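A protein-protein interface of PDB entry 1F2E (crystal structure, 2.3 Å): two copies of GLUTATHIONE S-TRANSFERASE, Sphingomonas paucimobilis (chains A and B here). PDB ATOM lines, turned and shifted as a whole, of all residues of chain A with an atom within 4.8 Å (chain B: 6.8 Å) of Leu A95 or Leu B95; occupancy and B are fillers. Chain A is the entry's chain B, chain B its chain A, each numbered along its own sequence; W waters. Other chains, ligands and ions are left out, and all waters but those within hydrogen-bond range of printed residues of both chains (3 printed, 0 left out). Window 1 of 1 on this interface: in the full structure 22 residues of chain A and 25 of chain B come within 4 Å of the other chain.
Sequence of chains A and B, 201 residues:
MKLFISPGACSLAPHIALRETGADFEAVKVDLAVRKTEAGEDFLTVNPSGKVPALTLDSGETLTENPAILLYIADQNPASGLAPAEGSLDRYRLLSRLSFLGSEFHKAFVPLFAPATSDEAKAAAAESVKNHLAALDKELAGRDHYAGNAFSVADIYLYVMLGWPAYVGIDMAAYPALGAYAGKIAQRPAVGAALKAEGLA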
ATOM      1  N   PRO A  67      14.230 -16.337  29.874  1.00  0.00           N
ATOM      2  CA  PRO A  67      14.643 -16.466  28.475  1.00  0.00           C
ATOM      3  C   PRO A  67      13.489 -16.266  27.489  1.00  0.00           C
ATOM      4  O   PRO A  67      13.630 -15.542  26.496  1.00  0.00           O
ATOM      5  CB  PRO A  67      15.223 -17.879  28.420  1.00  0.00           C
ATOM      6  CG  PRO A  67      15.781 -18.056  29.816  1.00  0.00           C
ATOM      7  CD  PRO A  67      14.656 -17.514  30.656  1.00  0.00           C
ATOM      8  N   ALA A  68      12.350 -16.901  27.772  1.00  0.00           N
ATOM      9  CA  ALA A  68      11.179 -16.800  26.899  1.00  0.00           C
ATOM     10  C   ALA A  68      10.576 -15.404  26.914  1.00  0.00           C
ATOM     11  O   ALA A  68      10.205 -14.865  25.870  1.00  0.00           O
ATOM     12  CB  ALA A  68      10.126 -17.823  27.310  1.00  0.00           C
ATOM     13  N   LEU A  71      13.102 -12.824  25.131  1.00  0.00           N
ATOM     14  CA  LEU A  71      13.049 -12.935  23.677  1.00  0.00           C
ATOM     15  C   LEU A  71      11.723 -12.415  23.142  1.00  0.00           C
ATOM     16  O   LEU A  71      11.683 -11.740  22.110  1.00  0.00           O
ATOM     17  CB  LEU A  71      13.260 -14.382  23.235  1.00  0.00           C
ATOM     18  CG  LEU A  71      14.734 -14.745  23.055  1.00  0.00           C
ATOM     19  CD1 LEU A  71      14.896 -16.240  22.875  1.00  0.00           C
ATOM     20  CD2 LEU A  71      15.283 -14.003  21.841  1.00  0.00           C
ATOM     21  N   ARG A  91      21.039 -15.912  16.651  1.00  0.00           N
ATOM     22  CA  ARG A  91      19.931 -16.090  17.556  1.00  0.00           C
ATOM     23  C   ARG A  91      20.181 -17.248  18.518  1.00  0.00           C
ATOM     24  O   ARG A  91      19.850 -17.162  19.700  1.00  0.00           O
ATOM     25  CB  ARG A  91      18.660 -16.321  16.751  1.00  0.00           C
ATOM     26  CG  ARG A  91      17.422 -15.977  17.508  1.00  0.00           C
ATOM     27  CD  ARG A  91      16.269 -15.751  16.575  1.00  0.00           C
ATOM     28  NE  ARG A  91      15.030 -15.672  17.336  1.00  0.00           N
ATOM     29  CZ  ARG A  91      14.569 -14.575  17.919  1.00  0.00           C
ATOM     30  NH1 ARG A  91      15.237 -13.432  17.828  1.00  0.00           N
ATOM     31  NH2 ARG A  91      13.434 -14.632  18.603  1.00  0.00           N
ATOM     32  N   TYR A  92      20.766 -18.328  18.013  1.00  0.00           N
ATOM     33  CA  TYR A  92      21.051 -19.489  18.852  1.00  0.00           C
ATOM     34  C   TYR A  92      22.124 -19.146  19.893  1.00  0.00           C
ATOM     35  O   TYR A  92      22.075 -19.629  21.030  1.00  0.00           O
ATOM     36  CB  TYR A  92      21.488 -20.677  17.977  1.00  0.00           C
ATOM     37  CG  TYR A  92      20.428 -21.047  16.966  1.00  0.00           C
ATOM     38  CD1 TYR A  92      20.495 -20.584  15.649  1.00  0.00           C
ATOM     39  CD2 TYR A  92      19.298 -21.774  17.353  1.00  0.00           C
ATOM     40  CE1 TYR A  92      19.459 -20.827  14.746  1.00  0.00           C
ATOM     41  CE2 TYR A  92      18.256 -22.021  16.462  1.00  0.00           C
ATOM     42  CZ  TYR A  92      18.342 -21.541  15.159  1.00  0.00           C
ATOM     43  OH  TYR A  92      17.300 -21.747  14.282  1.00  0.00           O
ATOM     44  N   ARG A  93      23.082 -18.303  19.504  1.00  0.00           N
ATOM     45  CA  ARG A  93      24.137 -17.881  20.420  1.00  0.00           C
ATOM     46  C   ARG A  93      23.454 -17.152  21.573  1.00  0.00           C
ATOM     47  O   ARG A  93      23.795 -17.356  22.737  1.00  0.00           O
ATOM     48  CB  ARG A  93      25.115 -16.924  19.729  1.00  0.00           C
ATOM     49  CG  ARG A  93      26.519 -16.919  20.336  1.00  0.00           C
ATOM     50  CD  ARG A  93      27.205 -15.536  20.287  1.00  0.00           C
ATOM     51  NE  ARG A  93      26.570 -14.618  19.346  1.00  0.00           N
ATOM     52  CZ  ARG A  93      27.213 -13.957  18.383  1.00  0.00           C
ATOM     53  NH1 ARG A  93      28.528 -14.112  18.226  1.00  0.00           N
ATOM     54  NH2 ARG A  93      26.537 -13.144  17.571  1.00  0.00           N
ATOM     55  N   LEU A  94      22.482 -16.306  21.239  1.00  0.00           N
ATOM     56  CA  LEU A  94      21.745 -15.541  22.246  1.00  0.00           C
ATOM     57  C   LEU A  94      21.004 -16.504  23.169  1.00  0.00           C
ATOM     58  O   LEU A  94      21.074 -16.393  24.394  1.00  0.00           O
ATOM     59  CB  LEU A  94      20.733 -14.597  21.576  1.00  0.00           C
ATOM     60  CG  LEU A  94      19.799 -13.827  22.529  1.00  0.00           C
ATOM     61  CD1 LEU A  94      20.637 -12.933  23.447  1.00  0.00           C
ATOM     62  CD2 LEU A  94      18.794 -12.983  21.730  1.00  0.00           C
ATOM     63  N   LEU A  95      20.303 -17.455  22.562  1.00  0.00           N
ATOM     64  CA  LEU A  95      19.543 -18.446  23.307  1.00  0.00           C
ATOM     65  C   LEU A  95      20.495 -19.175  24.255  1.00  0.00           C
ATOM     66  O   LEU A  95      20.189 -19.372  25.429  1.00  0.00           O
ATOM     67  CB  LEU A  95      18.889 -19.437  22.337  1.00  0.00           C
ATOM     68  CG  LEU A  95      17.614 -20.114  22.845  1.00  0.00           C
ATOM     69  CD1 LEU A  95      16.536 -19.059  23.043  1.00  0.00           C
ATOM     70  CD2 LEU A  95      17.139 -21.166  21.848  1.00  0.00           C
ATOM     71  N   SER A  96      21.656 -19.564  23.743  1.00  0.00           N
ATOM     72  CA  SER A  96      22.635 -20.255  24.568  1.00  0.00           C
ATOM     73  C   SER A  96      23.056 -19.388  25.756  1.00  0.00           C
ATOM     74  O   SER A  96      23.195 -19.883  26.871  1.00  0.00           O
ATOM     75  CB  SER A  96      23.864 -20.612  23.743  1.00  0.00           C
ATOM     76  OG  SER A  96      24.848 -21.215  24.564  1.00  0.00           O
ATOM     77  N   ARG A  97      23.256 -18.094  25.513  1.00  0.00           N
ATOM     78  CA  ARG A  97      23.657 -17.165  26.573  1.00  0.00           C
ATOM     79  C   ARG A  97      22.569 -17.021  27.635  1.00  0.00           C
ATOM     80  O   ARG A  97      22.845 -17.080  28.835  1.00  0.00           O
ATOM     81  CB  ARG A  97      23.987 -15.787  25.976  1.00  0.00           C
ATOM     82  CG  ARG A  97      25.223 -15.781  25.063  1.00  0.00           C
ATOM     83  CD  ARG A  97      26.495 -16.079  25.850  1.00  0.00           C
ATOM     84  NE  ARG A  97      27.503 -16.795  25.060  1.00  0.00           N
ATOM     85  CZ  ARG A  97      28.160 -16.287  24.020  1.00  0.00           C
ATOM     86  NH1 ARG A  97      27.925 -15.047  23.621  1.00  0.00           N
ATOM     87  NH2 ARG A  97      29.064 -17.018  23.381  1.00  0.00           N
ATOM     88  N   LEU A  98      21.332 -16.836  27.186  1.00  0.00           N
ATOM     89  CA  LEU A  98      20.207 -16.678  28.093  1.00  0.00           C
ATOM     90  C   LEU A  98      20.009 -17.929  28.933  1.00  0.00           C
ATOM     91  O   LEU A  98      19.638 -17.852  30.103  1.00  0.00           O
ATOM     92  CB  LEU A  98      18.933 -16.388  27.294  1.00  0.00           C
ATOM     93  CG  LEU A  98      18.931 -15.051  26.550  1.00  0.00           C
ATOM     94  CD1 LEU A  98      17.719 -14.981  25.649  1.00  0.00           C
ATOM     95  CD2 LEU A  98      18.926 -13.891  27.550  1.00  0.00           C
ATOM     96  N   SER A  99      20.259 -19.081  28.317  1.00  0.00           N
ATOM     97  CA  SER A  99      20.107 -20.369  28.967  1.00  0.00           C
ATOM     98  C   SER A  99      21.211 -20.633  29.992  1.00  0.00           C
ATOM     99  O   SER A  99      20.976 -21.237  31.039  1.00  0.00           O
ATOM    100  CB  SER A  99      20.092 -21.465  27.902  1.00  0.00           C
ATOM    101  OG  SER A  99      20.023 -22.741  28.498  1.00  0.00           O
ATOM    102  N   LEU B  63      27.982 -24.892  19.695  1.00  0.00           N
ATOM    103  CA  LEU B  63      26.857 -24.431  20.486  1.00  0.00           C
ATOM    104  C   LEU B  63      26.722 -25.232  21.778  1.00  0.00           C
ATOM    105  O   LEU B  63      26.926 -26.450  21.782  1.00  0.00           O
ATOM    106  CB  LEU B  63      25.598 -24.583  19.637  1.00  0.00           C
ATOM    107  CG  LEU B  63      24.295 -23.904  20.014  1.00  0.00           C
ATOM    108  CD1 LEU B  63      24.490 -22.390  20.031  1.00  0.00           C
ATOM    109  CD2 LEU B  63      23.233 -24.295  18.994  1.00  0.00           C
ATOM    110  N   THR B  64      26.401 -24.546  22.872  1.00  0.00           N
ATOM    111  CA  THR B  64      26.196 -25.210  24.155  1.00  0.00           C
ATOM    112  C   THR B  64      24.831 -24.835  24.730  1.00  0.00           C
ATOM    113  O   THR B  64      24.187 -23.886  24.258  1.00  0.00           O
ATOM    114  CB  THR B  64      27.281 -24.844  25.191  1.00  0.00           C
ATOM    115  OG1 THR B  64      27.262 -23.433  25.433  1.00  0.00           O
ATOM    116  CG2 THR B  64      28.667 -25.275  24.698  1.00  0.00           C
ATOM    117  N   GLU B  65      24.405 -25.594  25.743  1.00  0.00           N
ATOM    118  CA  GLU B  65      23.127 -25.405  26.431  1.00  0.00           C
ATOM    119  C   GLU B  65      21.997 -26.098  25.665  1.00  0.00           C
ATOM    120  O   GLU B  65      21.670 -25.725  24.542  1.00  0.00           O
ATOM    121  CB  GLU B  65      22.842 -23.909  26.623  1.00  0.00           C
ATOM    122  CG  GLU B  65      23.900 -23.191  27.483  1.00  0.00           C
ATOM    123  CD  GLU B  65      23.862 -23.607  28.956  1.00  0.00           C
ATOM    124  OE1 GLU B  65      24.917 -23.534  29.621  1.00  0.00           O
ATOM    125  OE2 GLU B  65      22.780 -23.995  29.460  1.00  0.00           O
ATOM    126  N   PRO B  67      18.647 -26.116  25.633  1.00  0.00           N
ATOM    127  CA  PRO B  67      17.559 -25.414  24.942  1.00  0.00           C
ATOM    128  C   PRO B  67      17.990 -24.890  23.570  1.00  0.00           C
ATOM    129  O   PRO B  67      17.280 -25.069  22.575  1.00  0.00           O
ATOM    130  CB  PRO B  67      17.205 -24.284  25.910  1.00  0.00           C
ATOM    131  CG  PRO B  67      17.562 -24.876  27.267  1.00  0.00           C
ATOM    132  CD  PRO B  67      18.891 -25.537  26.968  1.00  0.00           C
ATOM    133  N   ALA B  68      19.159 -24.252  23.517  1.00  0.00           N
ATOM    134  CA  ALA B  68      19.673 -23.690  22.269  1.00  0.00           C
ATOM    135  C   ALA B  68      19.960 -24.788  21.256  1.00  0.00           C
ATOM    136  O   ALA B  68      19.535 -24.715  20.105  1.00  0.00           O
ATOM    137  CB  ALA B  68      20.937 -22.877  22.540  1.00  0.00           C
ATOM    138  N   ILE B  69      20.680 -25.809  21.698  1.00  0.00           N
ATOM    139  CA  ILE B  69      21.018 -26.934  20.845  1.00  0.00           C
ATOM    140  C   ILE B  69      19.762 -27.631  20.334  1.00  0.00           C
ATOM    141  O   ILE B  69      19.641 -27.908  19.145  1.00  0.00           O
ATOM    142  CB  ILE B  69      21.888 -27.963  21.602  1.00  0.00           C
ATOM    143  CG1 ILE B  69      23.211 -27.317  22.017  1.00  0.00           C
ATOM    144  CG2 ILE B  69      22.144 -29.187  20.715  1.00  0.00           C
ATOM    145  CD1 ILE B  69      24.161 -28.265  22.740  1.00  0.00           C
ATOM    146  N   LEU B  71      16.693 -26.458  20.074  1.00  0.00           N
ATOM    147  CA  LEU B  71      15.958 -25.592  19.161  1.00  0.00           C
ATOM    148  C   LEU B  71      16.644 -25.577  17.793  1.00  0.00           C
ATOM    149  O   LEU B  71      15.986 -25.663  16.751  1.00  0.00           O
ATOM    150  CB  LEU B  71      15.878 -24.175  19.728  1.00  0.00           C
ATOM    151  CG  LEU B  71      14.835 -23.309  19.028  1.00  0.00           C
ATOM    152  CD1 LEU B  71      13.438 -23.872  19.323  1.00  0.00           C
ATOM    153  CD2 LEU B  71      14.952 -21.861  19.501  1.00  0.00           C
ATOM    154  N   TYR B  72      17.969 -25.473  17.799  1.00  0.00           N
ATOM    155  CA  TYR B  72      18.735 -25.465  16.561  1.00  0.00           C
ATOM    156  C   TYR B  72      18.510 -26.759  15.769  1.00  0.00           C
ATOM    157  O   TYR B  72      18.300 -26.728  14.555  1.00  0.00           O
ATOM    158  CB  TYR B  72      20.228 -25.300  16.863  1.00  0.00           C
ATOM    159  CG  TYR B  72      21.098 -25.306  15.625  1.00  0.00           C
ATOM    160  CD1 TYR B  72      21.512 -26.506  15.047  1.00  0.00           C
ATOM    161  CD2 TYR B  72      21.451 -24.112  14.990  1.00  0.00           C
ATOM    162  CE1 TYR B  72      22.250 -26.521  13.863  1.00  0.00           C
ATOM    163  CE2 TYR B  72      22.188 -24.114  13.802  1.00  0.00           C
ATOM    164  CZ  TYR B  72      22.584 -25.326  13.243  1.00  0.00           C
ATOM    165  OH  TYR B  72      23.303 -25.348  12.058  1.00  0.00           O
ATOM    166  N   PRO B  84       7.801 -25.235  17.090  1.00  0.00           N
ATOM    167  CA  PRO B  84       6.999 -24.326  16.269  1.00  0.00           C
ATOM    168  C   PRO B  84       7.876 -23.391  15.427  1.00  0.00           C
ATOM    169  O   PRO B  84       9.057 -23.203  15.717  1.00  0.00           O
ATOM    170  CB  PRO B  84       6.132 -23.583  17.297  1.00  0.00           C
ATOM    171  CG  PRO B  84       6.796 -23.851  18.633  1.00  0.00           C
ATOM    172  CD  PRO B  84       7.339 -25.241  18.487  1.00  0.00           C
ATOM    173  N   ASP B  90       3.495 -19.642  19.850  1.00  0.00           N
ATOM    174  CA  ASP B  90       3.753 -20.998  20.310  1.00  0.00           C
ATOM    175  C   ASP B  90       5.236 -21.294  20.487  1.00  0.00           C
ATOM    176  O   ASP B  90       5.602 -22.198  21.226  1.00  0.00           O
ATOM    177  CB  ASP B  90       3.127 -22.007  19.338  1.00  0.00           C
ATOM    178  CG  ASP B  90       3.042 -23.405  19.926  1.00  0.00           C
ATOM    179  OD1 ASP B  90       2.623 -23.528  21.095  1.00  0.00           O
ATOM    180  OD2 ASP B  90       3.380 -24.385  19.222  1.00  0.00           O
ATOM    181  N   ARG B  91       6.093 -20.531  19.819  1.00  0.00           N
ATOM    182  CA  ARG B  91       7.531 -20.752  19.938  1.00  0.00           C
ATOM    183  C   ARG B  91       8.030 -20.334  21.314  1.00  0.00           C
ATOM    184  O   ARG B  91       8.939 -20.956  21.877  1.00  0.00           O
ATOM    185  CB  ARG B  91       8.292 -19.976  18.860  1.00  0.00           C
ATOM    186  CG  ARG B  91       9.748 -20.408  18.724  1.00  0.00           C
ATOM    187  CD  ARG B  91      10.398 -19.772  17.512  1.00  0.00           C
ATOM    188  NE  ARG B  91      11.818 -20.092  17.418  1.00  0.00           N
ATOM    189  CZ  ARG B  91      12.317 -21.196  16.868  1.00  0.00           C
ATOM    190  NH1 ARG B  91      11.514 -22.115  16.345  1.00  0.00           N
ATOM    191  NH2 ARG B  91      13.631 -21.372  16.838  1.00  0.00           N
ATOM    192  N   TYR B  92       7.434 -19.277  21.854  1.00  0.00           N
ATOM    193  CA  TYR B  92       7.822 -18.793  23.167  1.00  0.00           C
ATOM    194  C   TYR B  92       7.345 -19.773  24.225  1.00  0.00           C
ATOM    195  O   TYR B  92       8.025 -19.983  25.236  1.00  0.00           O
ATOM    196  CB  TYR B  92       7.255 -17.386  23.401  1.00  0.00           C
ATOM    197  CG  TYR B  92       7.721 -16.413  22.335  1.00  0.00           C
ATOM    198  CD1 TYR B  92       6.937 -16.155  21.211  1.00  0.00           C
ATOM    199  CD2 TYR B  92       8.991 -15.829  22.402  1.00  0.00           C
ATOM    200  CE1 TYR B  92       7.403 -15.346  20.176  1.00  0.00           C
ATOM    201  CE2 TYR B  92       9.467 -15.019  21.369  1.00  0.00           C
ATOM    202  CZ  TYR B  92       8.666 -14.786  20.260  1.00  0.00           C
ATOM    203  OH  TYR B  92       9.132 -14.011  19.224  1.00  0.00           O
ATOM    204  N   ARG B  93       6.188 -20.388  23.989  1.00  0.00           N
ATOM    205  CA  ARG B  93       5.678 -21.384  24.929  1.00  0.00           C
ATOM    206  C   ARG B  93       6.716 -22.501  24.980  1.00  0.00           C
ATOM    207  O   ARG B  93       7.028 -23.013  26.046  1.00  0.00           O
ATOM    208  CB  ARG B  93       4.344 -21.974  24.462  1.00  0.00           C
ATOM    209  CG  ARG B  93       3.239 -20.959  24.261  1.00  0.00           C
ATOM    210  CD  ARG B  93       1.912 -21.643  23.966  1.00  0.00           C
ATOM    211  NE  ARG B  93       0.885 -20.664  23.625  1.00  0.00           N
ATOM    212  CZ  ARG B  93       0.386 -20.491  22.406  1.00  0.00           C
ATOM    213  NH1 ARG B  93       0.813 -21.242  21.396  1.00  0.00           N
ATOM    214  NH2 ARG B  93      -0.528 -19.555  22.194  1.00  0.00           N
ATOM    215  N   LEU B  94       7.249 -22.878  23.823  1.00  0.00           N
ATOM    216  CA  LEU B  94       8.258 -23.929  23.781  1.00  0.00           C
ATOM    217  C   LEU B  94       9.509 -23.488  24.531  1.00  0.00           C
ATOM    218  O   LEU B  94      10.056 -24.239  25.339  1.00  0.00           O
ATOM    219  CB  LEU B  94       8.644 -24.274  22.339  1.00  0.00           C
ATOM    220  CG  LEU B  94       9.822 -25.249  22.230  1.00  0.00           C
ATOM    221  CD1 LEU B  94       9.464 -26.569  22.940  1.00  0.00           C
ATOM    222  CD2 LEU B  94      10.152 -25.512  20.765  1.00  0.00           C
ATOM    223  N   LEU B  95       9.957 -22.267  24.264  1.00  0.00           N
ATOM    224  CA  LEU B  95      11.158 -21.754  24.915  1.00  0.00           C
ATOM    225  C   LEU B  95      11.006 -21.715  26.435  1.00  0.00           C
ATOM    226  O   LEU B  95      11.965 -21.965  27.179  1.00  0.00           O
ATOM    227  CB  LEU B  95      11.486 -20.362  24.379  1.00  0.00           C
ATOM    228  CG  LEU B  95      12.736 -19.715  24.975  1.00  0.00           C
ATOM    229  CD1 LEU B  95      13.931 -20.677  24.925  1.00  0.00           C
ATOM    230  CD2 LEU B  95      13.024 -18.440  24.205  1.00  0.00           C
ATOM    231  N   SER B  96       9.801 -21.401  26.892  1.00  0.00           N
ATOM    232  CA  SER B  96       9.524 -21.353  28.321  1.00  0.00           C
ATOM    233  C   SER B  96       9.681 -22.756  28.916  1.00  0.00           C
ATOM    234  O   SER B  96      10.286 -22.920  29.975  1.00  0.00           O
ATOM    235  CB  SER B  96       8.101 -20.834  28.560  1.00  0.00           C
ATOM    236  OG  SER B  96       7.698 -21.043  29.903  1.00  0.00           O
ATOM    237  N   ARG B  97       9.139 -23.763  28.223  1.00  0.00           N
ATOM    238  CA  ARG B  97       9.227 -25.144  28.688  1.00  0.00           C
ATOM    239  C   ARG B  97      10.665 -25.629  28.714  1.00  0.00           C
ATOM    240  O   ARG B  97      11.085 -26.282  29.669  1.00  0.00           O
ATOM    241  CB  ARG B  97       8.383 -26.085  27.809  1.00  0.00           C
ATOM    242  CG  ARG B  97       6.870 -25.950  27.995  1.00  0.00           C
ATOM    243  CD  ARG B  97       6.487 -25.962  29.474  1.00  0.00           C
ATOM    244  NE  ARG B  97       6.646 -24.638  30.086  1.00  0.00           N
ATOM    245  CZ  ARG B  97       6.703 -24.406  31.400  1.00  0.00           C
ATOM    246  NH1 ARG B  97       6.844 -23.164  31.850  1.00  0.00           N
ATOM    247  NH2 ARG B  97       6.637 -25.413  32.264  1.00  0.00           N
ATOM    248  N   LEU B  98      11.427 -25.317  27.670  1.00  0.00           N
ATOM    249  CA  LEU B  98      12.822 -25.745  27.639  1.00  0.00           C
ATOM    250  C   LEU B  98      13.581 -25.075  28.771  1.00  0.00           C
ATOM    251  O   LEU B  98      14.444 -25.683  29.421  1.00  0.00           O
ATOM    252  CB  LEU B  98      13.470 -25.384  26.305  1.00  0.00           C
ATOM    253  CG  LEU B  98      12.847 -26.041  25.068  1.00  0.00           C
ATOM    254  CD1 LEU B  98      13.603 -25.600  23.814  1.00  0.00           C
ATOM    255  CD2 LEU B  98      12.876 -27.554  25.222  1.00  0.00           C
ATOM    256  N   SER B  99      13.250 -23.814  29.008  1.00  0.00           N
ATOM    257  CA  SER B  99      13.897 -23.045  30.057  1.00  0.00           C
ATOM    258  C   SER B  99      13.588 -23.592  31.450  1.00  0.00           C
ATOM    259  O   SER B  99      14.471 -23.659  32.312  1.00  0.00           O
ATOM    260  CB  SER B  99      13.465 -21.583  29.963  1.00  0.00           C
ATOM    261  OG  SER B  99      13.887 -20.878  31.106  1.00  0.00           O
ATOM    262  N   PHE B 100      12.338 -23.983  31.674  1.00  0.00           N
ATOM    263  CA  PHE B 100      11.950 -24.520  32.972  1.00  0.00           C
ATOM    264  C   PHE B 100      12.670 -25.842  33.216  1.00  0.00           C
ATOM    265  O   PHE B 100      13.217 -26.080  34.292  1.00  0.00           O
ATOM    266  CB  PHE B 100      10.441 -24.755  33.030  1.00  0.00           C
ATOM    267  CG  PHE B 100       9.999 -25.509  34.251  1.00  0.00           C
ATOM    268  CD1 PHE B 100       9.821 -24.851  35.467  1.00  0.00           C
ATOM    269  CD2 PHE B 100       9.793 -26.882  34.196  1.00  0.00           C
ATOM    270  CE1 PHE B 100       9.445 -25.552  36.614  1.00  0.00           C
ATOM    271  CE2 PHE B 100       9.418 -27.600  35.338  1.00  0.00           C
ATOM    272  CZ  PHE B 100       9.243 -26.933  36.548  1.00  0.00           C
ATOM    273  N   ALA B 147       4.759 -29.360  25.654  1.00  0.00           N
ATOM    274  CA  ALA B 147       4.732 -28.013  25.099  1.00  0.00           C
ATOM    275  C   ALA B 147       3.882 -27.978  23.839  1.00  0.00           C
ATOM    276  O   ALA B 147       4.198 -28.624  22.835  1.00  0.00           O
ATOM    277  CB  ALA B 147       6.147 -27.551  24.777  1.00  0.00           C
HETATM  278  O   HOH W   1      13.968 -18.538  18.764  1.00  0.00           O
HETATM  279  O   HOH W   2      20.006 -24.662  30.047  1.00  0.00           O
HETATM  280  O   HOH W   3      27.010 -21.295  22.654  1.00  0.00           O
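Of chain B, only Pro B67, Ala B68, Leu B71 and Leu B95 come within 4 Å of Leu A95. Of the printed residues of chain A, Glu B65 touches Ser A96 (3.4 Å) and Ser A99 (3.2 Å). Of the printed residues of chain B, Pro A67 touches Leu B95 and Ser B99. Of the printed residues of chain A, Pro B67 touches Leu A95 (3.97 Å) and Ser A99 (3.4 Å). Of the printed residues of chain B, Leu A71 touches Tyr B92 and Leu B95.
Among the printed residues, merely in contact across the chains: Leu A71 with Leu B95 (3.2 Å), Leu A95 with Leu B71 (3.3 Å), Ser A99 with Pro B67 (3.4 Å), Ser A96 with Glu B65 (3.4 Å), Tyr A92 with Tyr B72 (3.5 Å), Pro A67 with Ser B99 (3.5 Å), Ser A96 with Ala B68 (3.6 Å), Leu A95 with Leu B95 (3.6 Å), Leu A95 with Ala B68 (3.6 Å), Ala A68 with Ser B96 (3.6 Å), Ala A68 with Leu B95 (3.7 Å), Ala A68 with Tyr B92 (3.7 Å), Pro A67 with Leu B95 (3.7 Å), Tyr A92 with Ala B68 (3.8 Å), Tyr A92 with Leu B63 (3.8 Å), Leu A71 with Tyr B92 (3.9 Å) and Leu A95 with Pro B67 (3.97 Å).
Water W2 bridges the side-chain hydroxyl of Ser A99 (2.5 Å) and the side-chain carboxylate of Glu B65 (2.9 Å). Water W3 bridges the side-chain hydroxyl (OG) of Ser A96 (2.9 Å) and the backbone NH (N) of Thr B64 (3.3 Å). Water W1 lies within hydrogen-bond range of NE of Arg B91 (3.0 Å) and NE of Arg A91 (3.4 Å).
Of the 12 printed residues of chain A, 7 touch a printed residue of chain B. Printed residues of chain B that touch a printed residue of chain A: Leu B63, Thr B64, Glu B65, Pro B67, Ala B68, Leu B71, Tyr B72, Tyr B92, Leu B95, Ser B96 and Ser B99. Hydrophobic or aromatic side chains of chain B that line the printed part of chain A: Leu B63, Pro B67, Ala B68, Leu B71, Tyr B72, Tyr B92 and Leu B95.
Pro A67 touches Leu B95, and with the chains exchanged Leu A95 touches Pro B67. Ala A68 touches Tyr B92, and with the chains exchanged Tyr A92 touches Ala B68. Leu A71 touches Leu B95, and with the chains exchanged Leu A95 touches Leu B71. Leu A95 touches its own counterpart, Leu B95. Of the 19 pairs that touch across the chains among the printed residues, 13 have their exchanged pair printed and touching as well.
The guanidinium group (NH1) of Arg B97 sits at hydrogen-bond distance from the side-chain hydroxyl (OG) of Ser B96 (3.0 Å).
OG of Ser A96 sits at hydrogen-bond distance from O of Thr B64, 2.8 Å away. The side-chain hydroxyl (OG) of Ser A99 sits at hydrogen-bond distance from the side-chain carboxylate (OE2) of Glu B65.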
